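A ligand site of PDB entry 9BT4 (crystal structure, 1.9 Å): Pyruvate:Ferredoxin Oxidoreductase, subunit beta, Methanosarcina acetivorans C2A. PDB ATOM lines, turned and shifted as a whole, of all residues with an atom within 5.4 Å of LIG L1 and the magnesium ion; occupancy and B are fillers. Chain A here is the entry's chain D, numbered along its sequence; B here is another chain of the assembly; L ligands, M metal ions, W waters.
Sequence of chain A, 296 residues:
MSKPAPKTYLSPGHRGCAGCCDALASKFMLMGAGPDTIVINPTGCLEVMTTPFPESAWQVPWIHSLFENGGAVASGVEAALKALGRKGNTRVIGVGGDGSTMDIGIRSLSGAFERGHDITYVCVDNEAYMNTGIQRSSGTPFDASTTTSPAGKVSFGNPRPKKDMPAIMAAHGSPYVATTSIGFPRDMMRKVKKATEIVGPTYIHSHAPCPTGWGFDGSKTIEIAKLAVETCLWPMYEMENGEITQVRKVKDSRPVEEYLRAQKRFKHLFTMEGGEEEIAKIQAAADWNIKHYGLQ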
ATOM      1  N   ARG A  15      28.211  31.470 -17.682  1.00  0.00           N
ATOM      2  CA  ARG A  15      28.226  31.227 -16.252  1.00  0.00           C
ATOM      3  C   ARG A  15      28.842  29.869 -15.924  1.00  0.00           C
ATOM      4  O   ARG A  15      28.563  29.311 -14.859  1.00  0.00           O
ATOM      5  CB  ARG A  15      26.808  31.309 -15.679  1.00  0.00           C
ATOM      6  CG  ARG A  15      26.260  32.694 -15.384  1.00  0.00           C
ATOM      7  CD  ARG A  15      26.074  33.558 -16.613  1.00  0.00           C
ATOM      8  NE  ARG A  15      25.225  34.715 -16.307  1.00  0.00           N
ATOM      9  CZ  ARG A  15      24.970  35.711 -17.147  1.00  0.00           C
ATOM     10  NH1 ARG A  15      25.574  35.749 -18.331  1.00  0.00           N
ATOM     11  NH2 ARG A  15      24.112  36.658 -16.811  1.00  0.00           N
ATOM     12  N   GLY A  16      29.704  29.348 -16.803  1.00  0.00           N
ATOM     13  CA  GLY A  16      30.379  28.088 -16.513  1.00  0.00           C
ATOM     14  C   GLY A  16      31.282  28.218 -15.293  1.00  0.00           C
ATOM     15  O   GLY A  16      31.845  29.275 -15.049  1.00  0.00           O
ATOM     16  N   CYS A  17      31.423  27.127 -14.521  1.00  0.00           N
ATOM     17  CA  CYS A  17      32.368  27.152 -13.408  1.00  0.00           C
ATOM     18  C   CYS A  17      33.751  27.519 -13.950  1.00  0.00           C
ATOM     19  O   CYS A  17      34.021  27.369 -15.138  1.00  0.00           O
ATOM     20  CB  CYS A  17      32.512  25.804 -12.720  1.00  0.00           C
ATOM     21  SG  CYS A  17      30.994  25.038 -12.093  1.00  0.00           S
ATOM     22  N   ALA A  18      34.626  27.999 -13.054  1.00  0.00           N
ATOM     23  CA  ALA A  18      36.032  28.150 -13.397  1.00  0.00           C
ATOM     24  C   ALA A  18      36.548  26.803 -13.915  1.00  0.00           C
ATOM     25  O   ALA A  18      36.417  25.789 -13.227  1.00  0.00           O
ATOM     26  CB  ALA A  18      36.816  28.623 -12.186  1.00  0.00           C
ATOM     27  N   GLY A  19      37.063  26.813 -15.150  1.00  0.00           N
ATOM     28  CA  GLY A  19      37.673  25.645 -15.753  1.00  0.00           C
ATOM     29  C   GLY A  19      36.654  24.674 -16.362  1.00  0.00           C
ATOM     30  O   GLY A  19      36.917  23.477 -16.434  1.00  0.00           O
ATOM     31  N   CYS A  20      35.518  25.210 -16.846  1.00  0.00           N
ATOM     32  CA  CYS A  20      34.385  24.403 -17.267  1.00  0.00           C
ATOM     33  C   CYS A  20      34.688  23.553 -18.499  1.00  0.00           C
ATOM     34  O   CYS A  20      35.099  24.072 -19.544  1.00  0.00           O
ATOM     35  CB  CYS A  20      33.186  25.293 -17.582  1.00  0.00           C
ATOM     36  SG  CYS A  20      31.720  24.341 -18.051  1.00  0.00           S
ATOM     37  N   CYS A  21      34.411  22.251 -18.382  1.00  0.00           N
ATOM     38  CA  CYS A  21      34.588  21.249 -19.432  1.00  0.00           C
ATOM     39  C   CYS A  21      33.561  21.413 -20.553  1.00  0.00           C
ATOM     40  O   CYS A  21      33.864  21.172 -21.718  1.00  0.00           O
ATOM     41  CB  CYS A  21      34.480  19.841 -18.861  1.00  0.00           C
ATOM     42  SG  CYS A  21      33.000  19.565 -17.842  1.00  0.00           S
ATOM     43  N   ASP A  22      32.332  21.832 -20.195  1.00  0.00           N
ATOM     44  CA  ASP A  22      31.275  22.040 -21.174  1.00  0.00           C
ATOM     45  C   ASP A  22      31.613  23.237 -22.063  1.00  0.00           C
ATOM     46  O   ASP A  22      31.371  23.185 -23.271  1.00  0.00           O
ATOM     47  CB  ASP A  22      29.906  22.179 -20.537  1.00  0.00           C
ATOM     48  CG  ASP A  22      29.226  20.890 -20.089  1.00  0.00           C
ATOM     49  OD1 ASP A  22      29.920  19.853 -19.998  1.00  0.00           O
ATOM     50  OD2 ASP A  22      28.002  20.929 -19.853  1.00  0.00           O
ATOM     51  N   CYS A  45      24.109  21.898 -18.335  1.00  0.00           N
ATOM     52  CA  CYS A  45      24.989  22.982 -17.901  1.00  0.00           C
ATOM     53  C   CYS A  45      25.280  23.908 -19.075  1.00  0.00           C
ATOM     54  O   CYS A  45      25.203  25.129 -18.918  1.00  0.00           O
ATOM     55  CB  CYS A  45      26.315  22.417 -17.424  1.00  0.00           C
ATOM     56  SG  CYS A  45      26.374  22.012 -15.660  1.00  0.00           S
ATOM     57  N   MET A  49      24.131  27.764 -18.838  1.00  0.00           N
ATOM     58  CA  MET A  49      25.201  28.691 -18.500  1.00  0.00           C
ATOM     59  C   MET A  49      25.403  29.714 -19.609  1.00  0.00           C
ATOM     60  O   MET A  49      25.944  30.797 -19.340  1.00  0.00           O
ATOM     61  CB  MET A  49      26.507  27.948 -18.197  1.00  0.00           C
ATOM     62  CG  MET A  49      27.247  27.460 -19.425  1.00  0.00           C
ATOM     63  SD  MET A  49      28.510  26.254 -18.982  1.00  0.00           S
ATOM     64  CE  MET A  49      29.587  26.466 -20.395  1.00  0.00           C
ATOM     65  N   GLY A  97      24.837  16.819 -23.306  1.00  0.00           N
ATOM     66  CA  GLY A  97      25.598  16.066 -22.323  1.00  0.00           C
ATOM     67  C   GLY A  97      25.310  14.570 -22.416  1.00  0.00           C
ATOM     68  O   GLY A  97      24.422  14.132 -23.157  1.00  0.00           O
ATOM     69  N   ASP A  98      26.067  13.806 -21.627  1.00  0.00           N
ATOM     70  CA  ASP A  98      25.930  12.360 -21.503  1.00  0.00           C
ATOM     71  C   ASP A  98      24.485  12.000 -21.166  1.00  0.00           C
ATOM     72  O   ASP A  98      23.900  11.103 -21.766  1.00  0.00           O
ATOM     73  CB  ASP A  98      26.956  11.810 -20.519  1.00  0.00           C
ATOM     74  CG  ASP A  98      27.033  12.524 -19.177  1.00  0.00           C
ATOM     75  OD1 ASP A  98      27.352  13.739 -19.149  1.00  0.00           O
ATOM     76  OD2 ASP A  98      26.751  11.859 -18.147  1.00  0.00           O
ATOM     77  N   GLY A  99      23.906  12.711 -20.189  1.00  0.00           N
ATOM     78  CA  GLY A  99      22.547  12.450 -19.741  1.00  0.00           C
ATOM     79  C   GLY A  99      21.532  12.630 -20.860  1.00  0.00           C
ATOM     80  O   GLY A  99      20.680  11.766 -21.094  1.00  0.00           O
ATOM     81  N   VAL A 124      28.818  15.646 -25.039  1.00  0.00           N
ATOM     82  CA  VAL A 124      29.766  16.176 -24.073  1.00  0.00           C
ATOM     83  C   VAL A 124      29.653  15.331 -22.807  1.00  0.00           C
ATOM     84  O   VAL A 124      28.764  15.563 -21.981  1.00  0.00           O
ATOM     85  CB  VAL A 124      29.537  17.673 -23.791  1.00  0.00           C
ATOM     86  CG1 VAL A 124      30.584  18.243 -22.837  1.00  0.00           C
ATOM     87  CG2 VAL A 124      29.494  18.499 -25.071  1.00  0.00           C
ATOM     88  N   ASP A 125      30.563  14.363 -22.654  1.00  0.00           N
ATOM     89  CA  ASP A 125      30.422  13.330 -21.640  1.00  0.00           C
ATOM     90  C   ASP A 125      31.250  13.680 -20.411  1.00  0.00           C
ATOM     91  O   ASP A 125      32.457  13.420 -20.383  1.00  0.00           O
ATOM     92  CB  ASP A 125      30.751  11.953 -22.200  1.00  0.00           C
ATOM     93  CG  ASP A 125      30.571  10.779 -21.233  1.00  0.00           C
ATOM     94  OD1 ASP A 125      30.141  11.004 -20.075  1.00  0.00           O
ATOM     95  OD2 ASP A 125      30.869   9.637 -21.655  1.00  0.00           O
ATOM     96  N   ASN A 126      30.582  14.226 -19.390  1.00  0.00           N
ATOM     97  CA  ASN A 126      31.213  14.503 -18.103  1.00  0.00           C
ATOM     98  C   ASN A 126      30.790  13.477 -17.047  1.00  0.00           C
ATOM     99  O   ASN A 126      30.996  13.710 -15.864  1.00  0.00           O
ATOM    100  CB  ASN A 126      31.044  15.968 -17.712  1.00  0.00           C
ATOM    101  CG  ASN A 126      29.590  16.380 -17.564  1.00  0.00           C
ATOM    102  OD1 ASN A 126      28.701  15.545 -17.394  1.00  0.00           O
ATOM    103  ND2 ASN A 126      29.349  17.687 -17.614  1.00  0.00           N
ATOM    104  N   GLU A 127      30.170  12.373 -17.481  1.00  0.00           N
ATOM    105  CA  GLU A 127      29.996  11.165 -16.690  1.00  0.00           C
ATOM    106  C   GLU A 127      29.082  11.372 -15.482  1.00  0.00           C
ATOM    107  O   GLU A 127      29.179  10.640 -14.489  1.00  0.00           O
ATOM    108  CB  GLU A 127      31.366  10.590 -16.308  1.00  0.00           C
ATOM    109  CG  GLU A 127      32.153  10.142 -17.532  1.00  0.00           C
ATOM    110  CD  GLU A 127      33.416   9.335 -17.271  1.00  0.00           C
ATOM    111  OE1 GLU A 127      33.939   9.360 -16.137  1.00  0.00           O
ATOM    112  OE2 GLU A 127      33.869   8.667 -18.226  1.00  0.00           O
ATOM    113  N   ALA A 128      28.174  12.356 -15.575  1.00  0.00           N
ATOM    114  CA  ALA A 128      27.085  12.562 -14.635  1.00  0.00           C
ATOM    115  C   ALA A 128      26.158  13.664 -15.169  1.00  0.00           C
ATOM    116  O   ALA A 128      26.469  14.327 -16.164  1.00  0.00           O
ATOM    117  CB  ALA A 128      27.621  12.901 -13.259  1.00  0.00           C
ATOM    118  N   TYR A 129      25.010  13.796 -14.501  1.00  0.00           N
ATOM    119  CA  TYR A 129      24.108  14.927 -14.704  1.00  0.00           C
ATOM    120  C   TYR A 129      24.607  16.070 -13.827  1.00  0.00           C
ATOM    121  O   TYR A 129      24.392  16.063 -12.610  1.00  0.00           O
ATOM    122  CB  TYR A 129      22.671  14.589 -14.279  1.00  0.00           C
ATOM    123  CG  TYR A 129      21.974  13.453 -15.016  1.00  0.00           C
ATOM    124  CD1 TYR A 129      21.515  13.602 -16.321  1.00  0.00           C
ATOM    125  CD2 TYR A 129      21.728  12.243 -14.380  1.00  0.00           C
ATOM    126  CE1 TYR A 129      20.857  12.578 -16.973  1.00  0.00           C
ATOM    127  CE2 TYR A 129      21.070  11.206 -15.026  1.00  0.00           C
ATOM    128  CZ  TYR A 129      20.651  11.361 -16.331  1.00  0.00           C
ATOM    129  OH  TYR A 129      20.005  10.351 -16.967  1.00  0.00           O
ATOM    130  N   MET A 130      25.270  17.064 -14.435  1.00  0.00           N
ATOM    131  CA  MET A 130      25.977  18.075 -13.665  1.00  0.00           C
ATOM    132  C   MET A 130      25.055  19.228 -13.279  1.00  0.00           C
ATOM    133  O   MET A 130      25.097  19.676 -12.136  1.00  0.00           O
ATOM    134  CB  MET A 130      27.238  18.578 -14.364  1.00  0.00           C
ATOM    135  CG  MET A 130      28.331  17.527 -14.462  1.00  0.00           C
ATOM    136  SD  MET A 130      28.563  16.604 -12.927  1.00  0.00           S
ATOM    137  CE  MET A 130      30.020  15.646 -13.361  1.00  0.00           C
ATOM    138  N   ASN A 131      24.236  19.717 -14.218  1.00  0.00           N
ATOM    139  CA  ASN A 131      23.452  20.918 -13.950  1.00  0.00           C
ATOM    140  C   ASN A 131      22.556  20.705 -12.720  1.00  0.00           C
ATOM    141  O   ASN A 131      22.330  21.641 -11.963  1.00  0.00           O
ATOM    142  CB  ASN A 131      22.621  21.371 -15.144  1.00  0.00           C
ATOM    143  CG  ASN A 131      22.088  22.768 -14.947  1.00  0.00           C
ATOM    144  OD1 ASN A 131      22.856  23.738 -14.962  1.00  0.00           O
ATOM    145  ND2 ASN A 131      20.778  22.905 -14.775  1.00  0.00           N
ATOM    146  N   CYS A 210      34.838  17.112 -15.414  1.00  0.00           N
ATOM    147  CA  CYS A 210      34.170  18.218 -14.762  1.00  0.00           C
ATOM    148  C   CYS A 210      34.824  18.444 -13.396  1.00  0.00           C
ATOM    149  O   CYS A 210      34.753  17.566 -12.541  1.00  0.00           O
ATOM    150  CB  CYS A 210      32.681  17.914 -14.609  1.00  0.00           C
ATOM    151  SG  CYS A 210      31.715  19.091 -13.627  1.00  0.00           S
ATOM    152  N   PRO A 211      35.476  19.599 -13.169  1.00  0.00           N
ATOM    153  CA  PRO A 211      36.147  19.861 -11.899  1.00  0.00           C
ATOM    154  C   PRO A 211      35.168  19.868 -10.730  1.00  0.00           C
ATOM    155  O   PRO A 211      35.462  19.308  -9.669  1.00  0.00           O
ATOM    156  CB  PRO A 211      36.874  21.211 -12.104  1.00  0.00           C
ATOM    157  CG  PRO A 211      36.152  21.856 -13.274  1.00  0.00           C
ATOM    158  CD  PRO A 211      35.609  20.718 -14.122  1.00  0.00           C
ATOM    159  N   THR A 212      33.994  20.476 -10.933  1.00  0.00           N
ATOM    160  CA  THR A 212      32.969  20.584  -9.893  1.00  0.00           C
ATOM    161  C   THR A 212      32.423  19.194  -9.553  1.00  0.00           C
ATOM    162  O   THR A 212      32.332  18.847  -8.378  1.00  0.00           O
ATOM    163  CB  THR A 212      31.874  21.550 -10.335  1.00  0.00           C
ATOM    164  OG1 THR A 212      32.552  22.783 -10.512  1.00  0.00           O
ATOM    165  CG2 THR A 212      30.782  21.746  -9.288  1.00  0.00           C
ATOM    166  N   GLY A 213      32.109  18.410 -10.593  1.00  0.00           N
ATOM    167  CA  GLY A 213      31.394  17.143 -10.427  1.00  0.00           C
ATOM    168  C   GLY A 213      32.303  15.966 -10.095  1.00  0.00           C
ATOM    169  O   GLY A 213      31.886  15.039  -9.390  1.00  0.00           O
ATOM    170  N   ARG B  42      27.667  27.810  -9.226  1.00  0.00           N
ATOM    171  CA  ARG B  42      28.823  27.695 -10.092  1.00  0.00           C
ATOM    172  C   ARG B  42      30.079  28.012  -9.296  1.00  0.00           C
ATOM    173  O   ARG B  42      30.109  28.982  -8.540  1.00  0.00           O
ATOM    174  CB  ARG B  42      28.703  28.645 -11.297  1.00  0.00           C
ATOM    175  CG  ARG B  42      27.434  28.543 -12.128  1.00  0.00           C
ATOM    176  CD  ARG B  42      27.264  27.196 -12.839  1.00  0.00           C
ATOM    177  NE  ARG B  42      26.072  27.214 -13.691  1.00  0.00           N
ATOM    178  CZ  ARG B  42      25.451  26.157 -14.198  1.00  0.00           C
ATOM    179  NH1 ARG B  42      25.906  24.935 -13.991  1.00  0.00           N
ATOM    180  NH2 ARG B  42      24.353  26.328 -14.917  1.00  0.00           N
HETATM  181 FE1  LIG L   1      30.453  23.492 -13.652  1.00  0.00          FE
HETATM  182 FE2  LIG L   1      30.888  23.175 -16.292  1.00  0.00          FE
HETATM  183 FE3  LIG L   1      28.557  22.232 -15.159  1.00  0.00          FE
HETATM  184 FE4  LIG L   1      30.963  20.965 -14.676  1.00  0.00          FE
HETATM  185  S1  LIG L   1      29.882  21.135 -16.673  1.00  0.00           S
HETATM  186  S2  LIG L   1      29.349  21.560 -13.145  1.00  0.00           S
HETATM  187  S3  LIG L   1      32.359  22.739 -14.645  1.00  0.00           S
HETATM  188  S4  LIG L   1      29.225  24.416 -15.331  1.00  0.00           S
HETATM  189  N1  LG2 L   2      13.699  15.405 -16.963  1.00  0.00           N
HETATM  190  C1  LG2 L   2      13.216  16.165 -17.958  1.00  0.00           C
HETATM  191  C2  LG2 L   2      12.159  15.568 -18.830  1.00  0.00           C
HETATM  192  N2  LG2 L   2      13.610  17.409 -18.228  1.00  0.00           N
HETATM  193  C3  LG2 L   2      14.554  17.948 -17.426  1.00  0.00           C
HETATM  194  N3  LG2 L   2      14.931  19.208 -17.715  1.00  0.00           N
HETATM  195  C4  LG2 L   2      15.138  17.220 -16.371  1.00  0.00           C
HETATM  196  C5  LG2 L   2      14.643  15.946 -16.174  1.00  0.00           C
HETATM  197  C6  LG2 L   2      16.184  17.780 -15.439  1.00  0.00           C
HETATM  198  N4  LG2 L   2      17.499  18.028 -16.031  1.00  0.00           N
HETATM  199  C7  LG2 L   2      17.799  19.145 -16.745  1.00  0.00           C
HETATM  200  S1  LG2 L   2      19.406  19.132 -17.199  1.00  0.00           S
HETATM  201  C8  LG2 L   2      19.763  17.677 -16.429  1.00  0.00           C
HETATM  202  C9  LG2 L   2      18.622  17.195 -15.822  1.00  0.00           C
HETATM  203  C10 LG2 L   2      18.545  15.926 -15.026  1.00  0.00           C
HETATM  204  C11 LG2 L   2      21.112  17.074 -16.414  1.00  0.00           C
HETATM  205  C12 LG2 L   2      21.886  17.293 -17.670  1.00  0.00           C
HETATM  206  O1  LG2 L   2      22.943  16.317 -17.643  1.00  0.00           O
HETATM  207  P1  LG2 L   2      23.821  16.102 -18.966  1.00  0.00           P
HETATM  208  O2  LG2 L   2      22.890  15.960 -20.122  1.00  0.00           O
HETATM  209  O3  LG2 L   2      24.894  15.095 -18.678  1.00  0.00           O
HETATM  210  O4  LG2 L   2      24.495  17.554 -19.056  1.00  0.00           O
HETATM  211  P2  LG2 L   2      25.517  18.261 -18.048  1.00  0.00           P
HETATM  212  O5  LG2 L   2      24.670  19.162 -17.176  1.00  0.00           O
HETATM  213  O6  LG2 L   2      26.462  19.001 -18.945  1.00  0.00           O
HETATM  214  O7  LG2 L   2      26.176  17.098 -17.302  1.00  0.00           O
HETATM  215 MG    MG M   1      26.775  15.248 -17.924  1.00  0.00          MG
HETATM  216  O   HOH W   1      27.487  16.584 -19.815  1.00  0.00           O
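The side-chain amide nitrogen of Asn 126 lies close to a sulfur (S1) of LIG L1. An iron atom (FE3) of LIG L1 is bound by the side-chain sulfur of Cys 45, at 2.3 Å. The backbone NH (N) of Cys 17 sits close to a sulfur (S4) of LIG L1. The side-chain sulfur (SG) of Cys 17 is bound to an iron atom (FE1) of LIG L1 (2.3 Å). An iron atom (FE2) of LIG L1 is bound by the side-chain sulfur (SG) of Cys 20 (2.3 Å). The side-chain sulfur (SG) of Cys 210 is bound to an iron atom (FE4) of LIG L1, 2.3 Å away. NH1 of Arg 42 of chain B sits close to S4 of LIG L1 (3.6 Å). S1 of LIG L1 sits close to SG of Cys 21 (3.7 Å). An oxygen (O3) of LG2 L2 lies close to the backbone NH (N) of Asp 98, 3.4 Å away. O5 of LG2 L2 is in hydrogen-bond range of N of Cys 45 (3.0 Å). The side-chain sulfur (SG) of Cys 45 lies close to an oxygen (O5) of LG2 L2. O6 of LG2 L2 lies close to OD2 of Asp 22 (2.6 Å). N of Met 130 sits close to O7 of LG2 L2, at 3.0 Å. The backbone NH of Gly 99 sits at hydrogen-bond distance from an oxygen (O2) of LG2 L2, 3.4 Å away. N of Asn 131 is in hydrogen-bond range of O5 of LG2 L2, at 3.0 Å.
ND2 of Asn 126 sits at hydrogen-bond distance from OD1 of Asp 22, 3.3 Å away. The backbone NH of Asp 98 sits at hydrogen-bond distance from the backbone carbonyl oxygen of Val 124 (3.2 Å). The side-chain sulfur of Cys 45 sits close to the guanidinium group of Arg 42 of chain B. The side-chain sulfur of Cys 17 sits close to the side-chain hydroxyl of Thr 212. SG of Cys 210 sits close to N of Thr 212 (3.8 Å). The side-chain sulfur (SG) of Cys 210 sits close to the backbone NH (N) of Gly 213 (3.1 Å). OD1 of Asp 22 sits at hydrogen-bond distance from SG of Cys 21. The side-chain amide oxygen (OD1) of Asn 131 sits at hydrogen-bond distance from the guanidinium group (NH2) of Arg 42 of chain B, at 3.0 Å.
OD1 of Asp 22 sits close to S1 of LIG L1, 3.6 Å away. CB of Met 130 touches S2 of LIG L1 (3.9 Å). Pro 211 touches LIG L1 (CD to S3, 3.9 Å). CB of Thr 212 touches S2 of LIG L1 (3.8 Å). Hydrophobic or aromatic side chains within 4 Å of LIG L1: Met 130 and Pro 211. Within 4 Å of LIG L1: Cys 17, Cys 20, Cys 21, Asp 22, Cys 45, Asn 126, Met 130, Cys 210, Pro 211, Thr 212 and Arg 42 of chain B.
Of the 26 residues printed, 3 come within 4 Å of the magnesium ion.
The magnesium ion is bound by O of Ala 128 (2.0 Å), OD1 of Asn 126 (2.0 Å), OD1 of Asp 98 (2.0 Å), O3 of LG2 L2 (2.0 Å), O7 of LG2 L2 (2.0 Å) and water W1 (2.4 Å). The magnesium ion has six donor atoms within binding distance.
Water W1 lies within hydrogen-bond range of the backbone carbonyl oxygen of Val 124 (2.7 Å), an oxygen (O6) of LG2 L2 (2.8 Å) and the side-chain amide nitrogen of Asn 126 (3.1 Å).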
